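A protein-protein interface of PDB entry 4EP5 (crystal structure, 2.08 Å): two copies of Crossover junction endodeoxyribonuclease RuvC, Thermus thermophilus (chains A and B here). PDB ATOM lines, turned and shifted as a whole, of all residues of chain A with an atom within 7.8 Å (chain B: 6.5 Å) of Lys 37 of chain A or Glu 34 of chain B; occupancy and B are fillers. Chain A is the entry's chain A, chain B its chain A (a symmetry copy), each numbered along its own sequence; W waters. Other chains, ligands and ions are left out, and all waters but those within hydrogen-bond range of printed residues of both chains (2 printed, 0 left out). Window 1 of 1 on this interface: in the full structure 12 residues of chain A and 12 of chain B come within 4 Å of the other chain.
OE1 of Glu 42 of chain A lies within salt-bridge range of NE of Arg 50 of chain B, at 3.9 Å.
ND1 of His 32 of chain B is in hydrogen-bond range of NH2 of Arg 140 of chain A (2.8 Å).
The guanidinium group (NE) of Arg 50 of chain B lies close to the guanidinium group (NE) of Arg 50 of chain A (3.5 Å).
The guanidinium group (NE) of Arg 54 of chain A lies within salt-bridge range of the side-chain carboxylate (OE1) of Glu 34 of chain A (2.9 Å).
The backbone NH of Ser 39 of chain A sits at hydrogen-bond distance from the side-chain carboxylate of Glu 42 of chain A (3.1 Å).
The side-chain carboxylate of Glu 42 of chain A lies within salt-bridge range of the guanidinium group of Arg 50 of chain A (2.7 Å).
The backbone NH of Glu 34 of chain B lies within hydrogen-bond range of the backbone carbonyl oxygen of Leu 15 of chain B (2.9 Å).
NE of Arg 54 of chain B is in salt-bridge range of OE1 of Glu 34 of chain B (2.9 Å).
O of Val 35 of chain B sits at hydrogen-bond distance from NZ of Lys 37 of chain B (2.7 Å).
Among the printed residues, pairs that only touch across the chains: Arg 54 of chain A with Lys 37 of chain B, Lys 37 of chain A with Arg 54 of chain B, Arg 140 of chain A with Phe 62 of chain B, Glu 34 of chain A with Lys 37 of chain B and Lys 37 of chain A with Glu 34 of chain B.
Lys 37 of chain A touches two residues of chain B.
Printed residues of chain B within 4 Å of Arg 140 of chain A: His 32 (2.8 Å) and Phe 62 (3.4 Å).
No residue of chain A comes within 4 Å of Gly 33 of chain B.
Glu 34 of chain B touches just one residue of chain A: Lys 37.
Of the printed residues of chain A, Lys 37 of chain B touches Glu 34 (3.9 Å) and Arg 54 (3.3 Å).
The nearest residue of chain A that does not touch Glu 34 of chain B is Arg 140 of chain A (6.3 Å).
Printed residues of chain A that touch a printed residue of chain B: Glu 34, Lys 37, Glu 42, Arg 50, Arg 54 and Arg 140.
Hydrophobic or aromatic side chains of chain B within 4 Å of the printed part of chain A: His 32 and Phe 62.
Among the printed residues, Asp or Glu carboxylates within 4 Å of a Lys or Arg side-chain nitrogen of the other chain: Glu 42 of chain A with Arg 50 of chain B.
Glu 34 of chain A touches Lys 37 of chain B, and with the chains exchanged Lys 37 of chain A touches Glu 34 of chain B.
Lys 37 of chain A touches Arg 54 of chain B, and with the chains exchanged Arg 54 of chain A touches Lys 37 of chain B.
Arg 50 of chain B touches its own counterpart, Arg 50 of chain A.
Positions printed for both chains: 13, 14, 33, 34, 35, 36, 37, 50 and 54.
Of the 8 pairs that touch across the chains among the printed residues, 5 have their exchanged pair printed and touching as well.
Water W2 bridges the backbone carbonyl oxygen of Lys 37 of chain A (2.8 Å) and the guanidinium group of Arg 50 of chain B (3.0 Å).
Water W1 lies within hydrogen-bond range of O of Lys 37 of chain B and NH2 of Arg 50 of chain A.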
ATOM      1  N   THR A  11     -11.200  -3.552  19.754  1.00  0.00           N
ATOM      2  CA  THR A  11     -10.797  -2.644  20.816  1.00  0.00           C
ATOM      3  C   THR A  11      -9.784  -1.620  20.300  1.00  0.00           C
ATOM      4  O   THR A  11      -9.280  -0.796  21.057  1.00  0.00           O
ATOM      5  CB  THR A  11     -10.199  -3.429  22.002  1.00  0.00           C
ATOM      6  OG1 THR A  11      -9.178  -2.649  22.631  1.00  0.00           O
ATOM      7  CG2 THR A  11      -9.589  -4.720  21.517  1.00  0.00           C
ATOM      8  N   HIS A  12      -9.502  -1.677  19.003  1.00  0.00           N
ATOM      9  CA  HIS A  12      -8.554  -0.768  18.372  1.00  0.00           C
ATOM     10  C   HIS A  12      -9.239  -0.216  17.139  1.00  0.00           C
ATOM     11  O   HIS A  12      -9.907  -0.957  16.434  1.00  0.00           O
ATOM     12  CB  HIS A  12      -7.296  -1.517  17.926  1.00  0.00           C
ATOM     13  CG  HIS A  12      -6.587  -2.246  19.021  1.00  0.00           C
ATOM     14  ND1 HIS A  12      -7.166  -3.278  19.728  1.00  0.00           N
ATOM     15  CD2 HIS A  12      -5.332  -2.114  19.514  1.00  0.00           C
ATOM     16  CE1 HIS A  12      -6.306  -3.736  20.619  1.00  0.00           C
ATOM     17  NE2 HIS A  12      -5.183  -3.048  20.510  1.00  0.00           N
ATOM     18  N   LEU A  13      -9.094   1.073  16.869  1.00  0.00           N
ATOM     19  CA  LEU A  13      -9.582   1.603  15.604  1.00  0.00           C
ATOM     20  C   LEU A  13      -8.435   2.265  14.840  1.00  0.00           C
ATOM     21  O   LEU A  13      -7.944   3.328  15.228  1.00  0.00           O
ATOM     22  CB  LEU A  13     -10.753   2.574  15.807  1.00  0.00           C
ATOM     23  CG  LEU A  13     -11.215   3.214  14.488  1.00  0.00           C
ATOM     24  CD1 LEU A  13     -12.718   3.124  14.320  1.00  0.00           C
ATOM     25  CD2 LEU A  13     -10.743   4.689  14.362  1.00  0.00           C
ATOM     26  N   GLY A  14      -7.999   1.620  13.760  1.00  0.00           N
ATOM     27  CA  GLY A  14      -6.910   2.133  12.964  1.00  0.00           C
ATOM     28  C   GLY A  14      -7.319   3.364  12.190  1.00  0.00           C
ATOM     29  O   GLY A  14      -8.363   3.387  11.537  1.00  0.00           O
ATOM     30  N   GLY A  33      -0.507   8.383  11.395  1.00  0.00           N
ATOM     31  CA  GLY A  33      -1.023   7.077  11.750  1.00  0.00           C
ATOM     32  C   GLY A  33      -1.232   6.996  13.247  1.00  0.00           C
ATOM     33  O   GLY A  33      -0.311   7.275  14.019  1.00  0.00           O
ATOM     34  N   GLU A  34      -2.444   6.629  13.653  1.00  0.00           N
ATOM     35  CA  GLU A  34      -2.754   6.400  15.060  1.00  0.00           C
ATOM     36  C   GLU A  34      -3.753   5.253  15.207  1.00  0.00           C
ATOM     37  O   GLU A  34      -4.452   4.889  14.250  1.00  0.00           O
ATOM     38  CB  GLU A  34      -3.304   7.673  15.730  1.00  0.00           C
ATOM     39  CG  GLU A  34      -4.695   8.061  15.287  1.00  0.00           C
ATOM     40  CD  GLU A  34      -5.224   9.324  15.973  1.00  0.00           C
ATOM     41  OE1 GLU A  34      -5.899   9.215  17.021  1.00  0.00           O
ATOM     42  OE2 GLU A  34      -4.984  10.427  15.450  1.00  0.00           O
ATOM     43  N   VAL A  35      -3.809   4.684  16.408  1.00  0.00           N
ATOM     44  CA  VAL A  35      -4.827   3.694  16.750  1.00  0.00           C
ATOM     45  C   VAL A  35      -5.617   4.182  17.970  1.00  0.00           C
ATOM     46  O   VAL A  35      -5.043   4.400  19.034  1.00  0.00           O
ATOM     47  CB  VAL A  35      -4.180   2.332  17.065  1.00  0.00           C
ATOM     48  CG1 VAL A  35      -5.212   1.337  17.578  1.00  0.00           C
ATOM     49  CG2 VAL A  35      -3.484   1.773  15.825  1.00  0.00           C
ATOM     50  N   VAL A  36      -6.922   4.381  17.813  1.00  0.00           N
ATOM     51  CA  VAL A  36      -7.779   4.655  18.964  1.00  0.00           C
ATOM     52  C   VAL A  36      -7.997   3.341  19.727  1.00  0.00           C
ATOM     53  O   VAL A  36      -8.606   2.398  19.207  1.00  0.00           O
ATOM     54  CB  VAL A  36      -9.133   5.267  18.544  1.00  0.00           C
ATOM     55  CG1 VAL A  36      -9.880   5.807  19.758  1.00  0.00           C
ATOM     56  CG2 VAL A  36      -8.922   6.390  17.538  1.00  0.00           C
ATOM     57  N   LYS A  37      -7.462   3.281  20.946  1.00  0.00           N
ATOM     58  CA  LYS A  37      -7.535   2.090  21.780  1.00  0.00           C
ATOM     59  C   LYS A  37      -8.555   2.284  22.893  1.00  0.00           C
ATOM     60  O   LYS A  37      -8.510   3.271  23.639  1.00  0.00           O
ATOM     61  CB  LYS A  37      -6.172   1.803  22.394  1.00  0.00           C
ATOM     62  CG  LYS A  37      -5.035   1.809  21.372  1.00  0.00           C
ATOM     63  CD  LYS A  37      -3.701   1.930  22.078  1.00  0.00           C
ATOM     64  CE  LYS A  37      -2.605   2.326  21.118  1.00  0.00           C
ATOM     65  NZ  LYS A  37      -2.873   3.668  20.543  1.00  0.00           N
ATOM     66  N   THR A  38      -9.478   1.337  22.998  1.00  0.00           N
ATOM     67  CA  THR A  38     -10.527   1.405  23.996  1.00  0.00           C
ATOM     68  C   THR A  38     -10.341   0.302  25.025  1.00  0.00           C
ATOM     69  O   THR A  38      -9.731  -0.723  24.737  1.00  0.00           O
ATOM     70  CB  THR A  38     -11.911   1.283  23.345  1.00  0.00           C
ATOM     71  OG1 THR A  38     -11.948   0.115  22.514  1.00  0.00           O
ATOM     72  CG2 THR A  38     -12.205   2.516  22.499  1.00  0.00           C
ATOM     73  N   SER A  39     -10.872   0.523  26.222  1.00  0.00           N
ATOM     74  CA  SER A  39     -10.733  -0.425  27.325  1.00  0.00           C
ATOM     75  C   SER A  39     -12.069  -1.081  27.636  1.00  0.00           C
ATOM     76  O   SER A  39     -13.125  -0.521  27.334  1.00  0.00           O
ATOM     77  CB  SER A  39     -10.215   0.293  28.576  1.00  0.00           C
ATOM     78  OG  SER A  39      -9.009   0.997  28.315  1.00  0.00           O
ATOM     79  N   GLU A  42     -14.074   1.205  30.352  1.00  0.00           N
ATOM     80  CA  GLU A  42     -14.704   2.481  30.015  1.00  0.00           C
ATOM     81  C   GLU A  42     -16.045   2.253  29.319  1.00  0.00           C
ATOM     82  O   GLU A  42     -16.192   1.334  28.515  1.00  0.00           O
ATOM     83  CB  GLU A  42     -13.773   3.402  29.200  1.00  0.00           C
ATOM     84  CG  GLU A  42     -13.403   2.892  27.839  1.00  0.00           C
ATOM     85  CD  GLU A  42     -12.592   3.899  27.019  1.00  0.00           C
ATOM     86  OE1 GLU A  42     -12.597   5.112  27.339  1.00  0.00           O
ATOM     87  OE2 GLU A  42     -11.947   3.469  26.048  1.00  0.00           O
ATOM     88  N   ARG A  47     -16.092   5.216  24.654  1.00  0.00           N
ATOM     89  CA  ARG A  47     -15.384   4.526  23.590  1.00  0.00           C
ATOM     90  C   ARG A  47     -15.783   5.095  22.237  1.00  0.00           C
ATOM     91  O   ARG A  47     -14.928   5.472  21.452  1.00  0.00           O
ATOM     92  CB  ARG A  47     -15.647   3.026  23.658  1.00  0.00           C
ATOM     93  CG  ARG A  47     -15.244   2.431  24.989  1.00  0.00           C
ATOM     94  CD  ARG A  47     -14.966   0.942  24.910  1.00  0.00           C
ATOM     95  NE  ARG A  47     -16.174   0.146  25.058  1.00  0.00           N
ATOM     96  CZ  ARG A  47     -16.893  -0.304  24.038  1.00  0.00           C
ATOM     97  NH1 ARG A  47     -17.982  -1.029  24.264  1.00  0.00           N
ATOM     98  NH2 ARG A  47     -16.517  -0.031  22.792  1.00  0.00           N
ATOM     99  N   ARG A  50     -14.892   9.043  21.917  1.00  0.00           N
ATOM    100  CA  ARG A  50     -13.471   9.289  21.651  1.00  0.00           C
ATOM    101  C   ARG A  50     -13.142   9.026  20.197  1.00  0.00           C
ATOM    102  O   ARG A  50     -12.405   9.787  19.572  1.00  0.00           O
ATOM    103  CB  ARG A  50     -12.581   8.432  22.550  1.00  0.00           C
ATOM    104  CG  ARG A  50     -12.611   8.864  24.003  1.00  0.00           C
ATOM    105  CD  ARG A  50     -11.371   8.412  24.755  1.00  0.00           C
ATOM    106  NE  ARG A  50     -11.295   6.962  24.838  1.00  0.00           N
ATOM    107  CZ  ARG A  50     -10.420   6.216  24.173  1.00  0.00           C
ATOM    108  NH1 ARG A  50     -10.436   4.902  24.325  1.00  0.00           N
ATOM    109  NH2 ARG A  50      -9.523   6.780  23.367  1.00  0.00           N
ATOM    110  N   ILE A  51     -13.680   7.936  19.662  1.00  0.00           N
ATOM    111  CA  ILE A  51     -13.462   7.602  18.264  1.00  0.00           C
ATOM    112  C   ILE A  51     -13.899   8.774  17.410  1.00  0.00           C
ATOM    113  O   ILE A  51     -13.160   9.233  16.536  1.00  0.00           O
ATOM    114  CB  ILE A  51     -14.231   6.346  17.849  1.00  0.00           C
ATOM    115  CG1 ILE A  51     -13.626   5.115  18.530  1.00  0.00           C
ATOM    116  CG2 ILE A  51     -14.199   6.199  16.336  1.00  0.00           C
ATOM    117  CD1 ILE A  51     -14.233   3.792  18.079  1.00  0.00           C
ATOM    118  N   ARG A  54     -11.461  11.756  17.832  1.00  0.00           N
ATOM    119  CA  ARG A  54     -10.198  11.508  17.155  1.00  0.00           C
ATOM    120  C   ARG A  54     -10.335  11.617  15.630  1.00  0.00           C
ATOM    121  O   ARG A  54      -9.526  12.275  14.981  1.00  0.00           O
ATOM    122  CB  ARG A  54      -9.619  10.144  17.552  1.00  0.00           C
ATOM    123  CG  ARG A  54      -8.984  10.123  18.939  1.00  0.00           C
ATOM    124  CD  ARG A  54      -8.191  11.398  19.211  1.00  0.00           C
ATOM    125  NE  ARG A  54      -7.096  11.597  18.265  1.00  0.00           N
ATOM    126  CZ  ARG A  54      -6.407  12.729  18.142  1.00  0.00           C
ATOM    127  NH1 ARG A  54      -6.692  13.777  18.911  1.00  0.00           N
ATOM    128  NH2 ARG A  54      -5.424  12.812  17.252  1.00  0.00           N
ATOM    129  N   ARG A 140       2.883  -1.180  12.085  1.00  0.00           N
ATOM    130  CA  ARG A 140       2.254  -1.920  13.168  1.00  0.00           C
ATOM    131  C   ARG A 140       1.389  -0.935  13.965  1.00  0.00           C
ATOM    132  O   ARG A 140       1.737   0.242  14.068  1.00  0.00           O
ATOM    133  CB  ARG A 140       3.354  -2.536  14.049  1.00  0.00           C
ATOM    134  CG  ARG A 140       2.887  -3.511  15.131  1.00  0.00           C
ATOM    135  CD  ARG A 140       2.589  -2.803  16.448  1.00  0.00           C
ATOM    136  NE  ARG A 140       3.804  -2.497  17.193  1.00  0.00           N
ATOM    137  CZ  ARG A 140       3.893  -1.550  18.120  1.00  0.00           C
ATOM    138  NH1 ARG A 140       2.836  -0.805  18.412  1.00  0.00           N
ATOM    139  NH2 ARG A 140       5.042  -1.347  18.750  1.00  0.00           N
ATOM    140  N   PRO A 141       0.255  -1.397  14.529  1.00  0.00           N
ATOM    141  CA  PRO A 141      -0.351  -2.732  14.476  1.00  0.00           C
ATOM    142  C   PRO A 141      -1.287  -2.942  13.294  1.00  0.00           C
ATOM    143  O   PRO A 141      -1.427  -2.062  12.445  1.00  0.00           O
ATOM    144  CB  PRO A 141      -1.134  -2.807  15.791  1.00  0.00           C
ATOM    145  CG  PRO A 141      -1.536  -1.397  16.052  1.00  0.00           C
ATOM    146  CD  PRO A 141      -0.413  -0.538  15.528  1.00  0.00           C
ATOM    147  N   LEU B  13      -0.474  12.197  26.724  1.00  0.00           N
ATOM    148  CA  LEU B  13       0.622  11.632  27.495  1.00  0.00           C
ATOM    149  C   LEU B  13       1.559  10.850  26.574  1.00  0.00           C
ATOM    150  O   LEU B  13       1.207   9.778  26.073  1.00  0.00           O
ATOM    151  CB  LEU B  13       0.115  10.758  28.650  1.00  0.00           C
ATOM    152  CG  LEU B  13       1.264  10.078  29.414  1.00  0.00           C
ATOM    153  CD1 LEU B  13       1.125  10.263  30.912  1.00  0.00           C
ATOM    154  CD2 LEU B  13       1.381   8.569  29.064  1.00  0.00           C
ATOM    155  N   GLY B  14       2.747  11.402  26.338  1.00  0.00           N
ATOM    156  CA  GLY B  14       3.712  10.769  25.470  1.00  0.00           C
ATOM    157  C   GLY B  14       4.298   9.529  26.101  1.00  0.00           C
ATOM    158  O   GLY B  14       4.720   9.541  27.259  1.00  0.00           O
ATOM    159  N   LEU B  15       4.349   8.453  25.327  1.00  0.00           N
ATOM    160  CA  LEU B  15       4.835   7.174  25.829  1.00  0.00           C
ATOM    161  C   LEU B  15       5.635   6.467  24.740  1.00  0.00           C
ATOM    162  O   LEU B  15       5.088   6.087  23.703  1.00  0.00           O
ATOM    163  CB  LEU B  15       3.655   6.315  26.278  1.00  0.00           C
ATOM    164  CG  LEU B  15       3.810   4.809  26.544  1.00  0.00           C
ATOM    165  CD1 LEU B  15       4.722   4.484  27.729  1.00  0.00           C
ATOM    166  CD2 LEU B  15       2.446   4.213  26.771  1.00  0.00           C
ATOM    167  N   GLY B  16       6.934   6.316  24.969  1.00  0.00           N
ATOM    168  CA  GLY B  16       7.810   5.705  23.992  1.00  0.00           C
ATOM    169  C   GLY B  16       8.795   4.711  24.578  1.00  0.00           C
ATOM    170  O   GLY B  16       9.165   4.799  25.754  1.00  0.00           O
ATOM    171  N   HIS B  32       8.661   1.530  20.083  1.00  0.00           N
ATOM    172  CA  HIS B  32       7.261   1.908  20.245  1.00  0.00           C
ATOM    173  C   HIS B  32       7.122   3.390  20.520  1.00  0.00           C
ATOM    174  O   HIS B  32       7.887   3.968  21.290  1.00  0.00           O
ATOM    175  CB  HIS B  32       6.647   1.135  21.414  1.00  0.00           C
ATOM    176  CG  HIS B  32       5.157   1.254  21.515  1.00  0.00           C
ATOM    177  ND1 HIS B  32       4.297   0.579  20.678  1.00  0.00           N
ATOM    178  CD2 HIS B  32       4.374   1.949  22.378  1.00  0.00           C
ATOM    179  CE1 HIS B  32       3.048   0.854  21.015  1.00  0.00           C
ATOM    180  NE2 HIS B  32       3.066   1.685  22.041  1.00  0.00           N
ATOM    181  N   GLY B  33       6.127   4.010  19.902  1.00  0.00           N
ATOM    182  CA  GLY B  33       5.765   5.366  20.258  1.00  0.00           C
ATOM    183  C   GLY B  33       4.267   5.547  20.143  1.00  0.00           C
ATOM    184  O   GLY B  33       3.684   5.248  19.099  1.00  0.00           O
ATOM    185  N   GLU B  34       3.647   6.020  21.221  1.00  0.00           N
ATOM    186  CA  GLU B  34       2.225   6.349  21.215  1.00  0.00           C
ATOM    187  C   GLU B  34       1.957   7.569  22.094  1.00  0.00           C
ATOM    188  O   GLU B  34       2.772   7.926  22.956  1.00  0.00           O
ATOM    189  CB  GLU B  34       1.370   5.156  21.684  1.00  0.00           C
ATOM    190  CG  GLU B  34       1.489   4.842  23.155  1.00  0.00           C
ATOM    191  CD  GLU B  34       0.622   3.660  23.598  1.00  0.00           C
ATOM    192  OE1 GLU B  34      -0.533   3.874  24.032  1.00  0.00           O
ATOM    193  OE2 GLU B  34       1.105   2.515  23.537  1.00  0.00           O
ATOM    194  N   VAL B  35       0.812   8.207  21.865  1.00  0.00           N
ATOM    195  CA  VAL B  35       0.338   9.283  22.731  1.00  0.00           C
ATOM    196  C   VAL B  35      -1.050   8.921  23.275  1.00  0.00           C
ATOM    197  O   VAL B  35      -1.986   8.724  22.502  1.00  0.00           O
ATOM    198  CB  VAL B  35       0.257  10.612  21.956  1.00  0.00           C
ATOM    199  CG1 VAL B  35      -0.387  11.704  22.800  1.00  0.00           C
ATOM    200  CG2 VAL B  35       1.651  11.050  21.506  1.00  0.00           C
ATOM    201  N   VAL B  36      -1.179   8.805  24.592  1.00  0.00           N
ATOM    202  CA  VAL B  36      -2.498   8.656  25.202  1.00  0.00           C
ATOM    203  C   VAL B  36      -3.197  10.024  25.180  1.00  0.00           C
ATOM    204  O   VAL B  36      -2.749  10.975  25.831  1.00  0.00           O
ATOM    205  CB  VAL B  36      -2.410   8.117  26.646  1.00  0.00           C
ATOM    206  CG1 VAL B  36      -3.786   7.700  27.151  1.00  0.00           C
ATOM    207  CG2 VAL B  36      -1.462   6.927  26.715  1.00  0.00           C
ATOM    208  N   LYS B  37      -4.272  10.114  24.399  1.00  0.00           N
ATOM    209  CA  LYS B  37      -5.019  11.352  24.228  1.00  0.00           C
ATOM    210  C   LYS B  37      -6.327  11.293  25.002  1.00  0.00           C
ATOM    211  O   LYS B  37      -7.116  10.349  24.856  1.00  0.00           O
ATOM    212  CB  LYS B  37      -5.317  11.578  22.753  1.00  0.00           C
ATOM    213  CG  LYS B  37      -4.086  11.436  21.857  1.00  0.00           C
ATOM    214  CD  LYS B  37      -4.509  11.262  20.414  1.00  0.00           C
ATOM    215  CE  LYS B  37      -3.374  10.737  19.568  1.00  0.00           C
ATOM    216  NZ  LYS B  37      -2.961   9.386  20.026  1.00  0.00           N
ATOM    217  N   ARG B  50      -7.150   4.947  31.772  1.00  0.00           N
ATOM    218  CA  ARG B  50      -6.616   4.589  30.455  1.00  0.00           C
ATOM    219  C   ARG B  50      -5.110   4.745  30.424  1.00  0.00           C
ATOM    220  O   ARG B  50      -4.401   3.901  29.880  1.00  0.00           O
ATOM    221  CB  ARG B  50      -7.249   5.430  29.350  1.00  0.00           C
ATOM    222  CG  ARG B  50      -8.704   5.085  29.098  1.00  0.00           C
ATOM    223  CD  ARG B  50      -9.152   5.491  27.705  1.00  0.00           C
ATOM    224  NE  ARG B  50      -9.117   6.934  27.531  1.00  0.00           N
ATOM    225  CZ  ARG B  50      -8.236   7.579  26.774  1.00  0.00           C
ATOM    226  NH1 ARG B  50      -8.296   8.897  26.684  1.00  0.00           N
ATOM    227  NH2 ARG B  50      -7.303   6.909  26.100  1.00  0.00           N
ATOM    228  N   ARG B  54      -2.645   1.776  29.435  1.00  0.00           N
ATOM    229  CA  ARG B  54      -1.708   1.897  28.329  1.00  0.00           C
ATOM    230  C   ARG B  54      -0.254   1.712  28.789  1.00  0.00           C
ATOM    231  O   ARG B  54       0.499   0.964  28.173  1.00  0.00           O
ATOM    232  CB  ARG B  54      -1.880   3.238  27.604  1.00  0.00           C
ATOM    233  CG  ARG B  54      -3.102   3.293  26.691  1.00  0.00           C
ATOM    234  CD  ARG B  54      -3.294   1.983  25.932  1.00  0.00           C
ATOM    235  NE  ARG B  54      -2.159   1.656  25.073  1.00  0.00           N
ATOM    236  CZ  ARG B  54      -1.975   0.472  24.490  1.00  0.00           C
ATOM    237  NH1 ARG B  54      -2.858  -0.508  24.667  1.00  0.00           N
ATOM    238  NH2 ARG B  54      -0.910   0.272  23.722  1.00  0.00           N
ATOM    239  N   VAL B  55       0.133   2.376  29.875  1.00  0.00           N
ATOM    240  CA  VAL B  55       1.501   2.262  30.375  1.00  0.00           C
ATOM    241  C   VAL B  55       1.812   0.833  30.803  1.00  0.00           C
ATOM    242  O   VAL B  55       2.859   0.286  30.461  1.00  0.00           O
ATOM    243  CB  VAL B  55       1.783   3.225  31.554  1.00  0.00           C
ATOM    244  CG1 VAL B  55       3.204   3.003  32.083  1.00  0.00           C
ATOM    245  CG2 VAL B  55       1.602   4.685  31.121  1.00  0.00           C
ATOM    246  N   VAL B  58       2.299  -1.352  27.867  1.00  0.00           N
ATOM    247  CA  VAL B  58       3.582  -1.116  27.229  1.00  0.00           C
ATOM    248  C   VAL B  58       4.734  -1.744  28.023  1.00  0.00           C
ATOM    249  O   VAL B  58       5.596  -2.398  27.454  1.00  0.00           O
ATOM    250  CB  VAL B  58       3.814   0.375  26.951  1.00  0.00           C
ATOM    251  CG1 VAL B  58       5.274   0.620  26.604  1.00  0.00           C
ATOM    252  CG2 VAL B  58       2.900   0.819  25.814  1.00  0.00           C
ATOM    253  N   PHE B  62       6.934  -4.659  26.448  1.00  0.00           N
ATOM    254  CA  PHE B  62       8.289  -4.308  26.022  1.00  0.00           C
ATOM    255  C   PHE B  62       9.371  -4.560  27.055  1.00  0.00           C
ATOM    256  O   PHE B  62      10.555  -4.531  26.720  1.00  0.00           O
ATOM    257  CB  PHE B  62       8.345  -2.875  25.495  1.00  0.00           C
ATOM    258  CG  PHE B  62       7.611  -2.689  24.200  1.00  0.00           C
ATOM    259  CD1 PHE B  62       8.202  -3.038  22.996  1.00  0.00           C
ATOM    260  CD2 PHE B  62       6.320  -2.187  24.191  1.00  0.00           C
ATOM    261  CE1 PHE B  62       7.524  -2.879  21.799  1.00  0.00           C
ATOM    262  CE2 PHE B  62       5.636  -2.020  23.002  1.00  0.00           C
ATOM    263  CZ  PHE B  62       6.239  -2.361  21.802  1.00  0.00           C
ATOM    264  N   HIS B 143       4.829  15.780  22.825  1.00  0.00           N
ATOM    265  CA  HIS B 143       4.773  14.875  23.964  1.00  0.00           C
ATOM    266  C   HIS B 143       5.452  13.545  23.686  1.00  0.00           C
ATOM    267  O   HIS B 143       6.077  12.969  24.572  1.00  0.00           O
ATOM    268  CB  HIS B 143       3.332  14.658  24.408  1.00  0.00           C
ATOM    269  CG  HIS B 143       2.722  15.859  25.055  1.00  0.00           C
ATOM    270  ND1 HIS B 143       2.396  15.898  26.395  1.00  0.00           N
ATOM    271  CD2 HIS B 143       2.390  17.070  24.550  1.00  0.00           C
ATOM    272  CE1 HIS B 143       1.882  17.079  26.684  1.00  0.00           C
ATOM    273  NE2 HIS B 143       1.870  17.811  25.583  1.00  0.00           N
ATOM    274  N   LEU B 144       5.329  13.054  22.458  1.00  0.00           N
ATOM    275  CA  LEU B 144       6.070  11.860  22.064  1.00  0.00           C
ATOM    276  C   LEU B 144       7.562  12.156  21.908  1.00  0.00           C
ATOM    277  O   LEU B 144       8.398  11.359  22.332  1.00  0.00           O
ATOM    278  CB  LEU B 144       5.521  11.262  20.770  1.00  0.00           C
ATOM    279  CG  LEU B 144       6.220   9.978  20.301  1.00  0.00           C
ATOM    280  CD1 LEU B 144       6.183   8.903  21.389  1.00  0.00           C
ATOM    281  CD2 LEU B 144       5.556   9.458  19.039  1.00  0.00           C
ATOM    282  N   ALA B 147       8.950  12.405  25.443  1.00  0.00           N
ATOM    283  CA  ALA B 147       9.091  11.070  26.027  1.00  0.00           C
ATOM    284  C   ALA B 147      10.279  10.263  25.473  1.00  0.00           C
ATOM    285  O   ALA B 147      10.943   9.542  26.217  1.00  0.00           O
ATOM    286  CB  ALA B 147       7.796  10.291  25.882  1.00  0.00           C
HETATM  287  O   HOH W   1      -8.744   9.605  22.693  1.00  0.00           O
HETATM  288  O   HOH W   2      -6.681   4.003  25.640  1.00  0.00           O
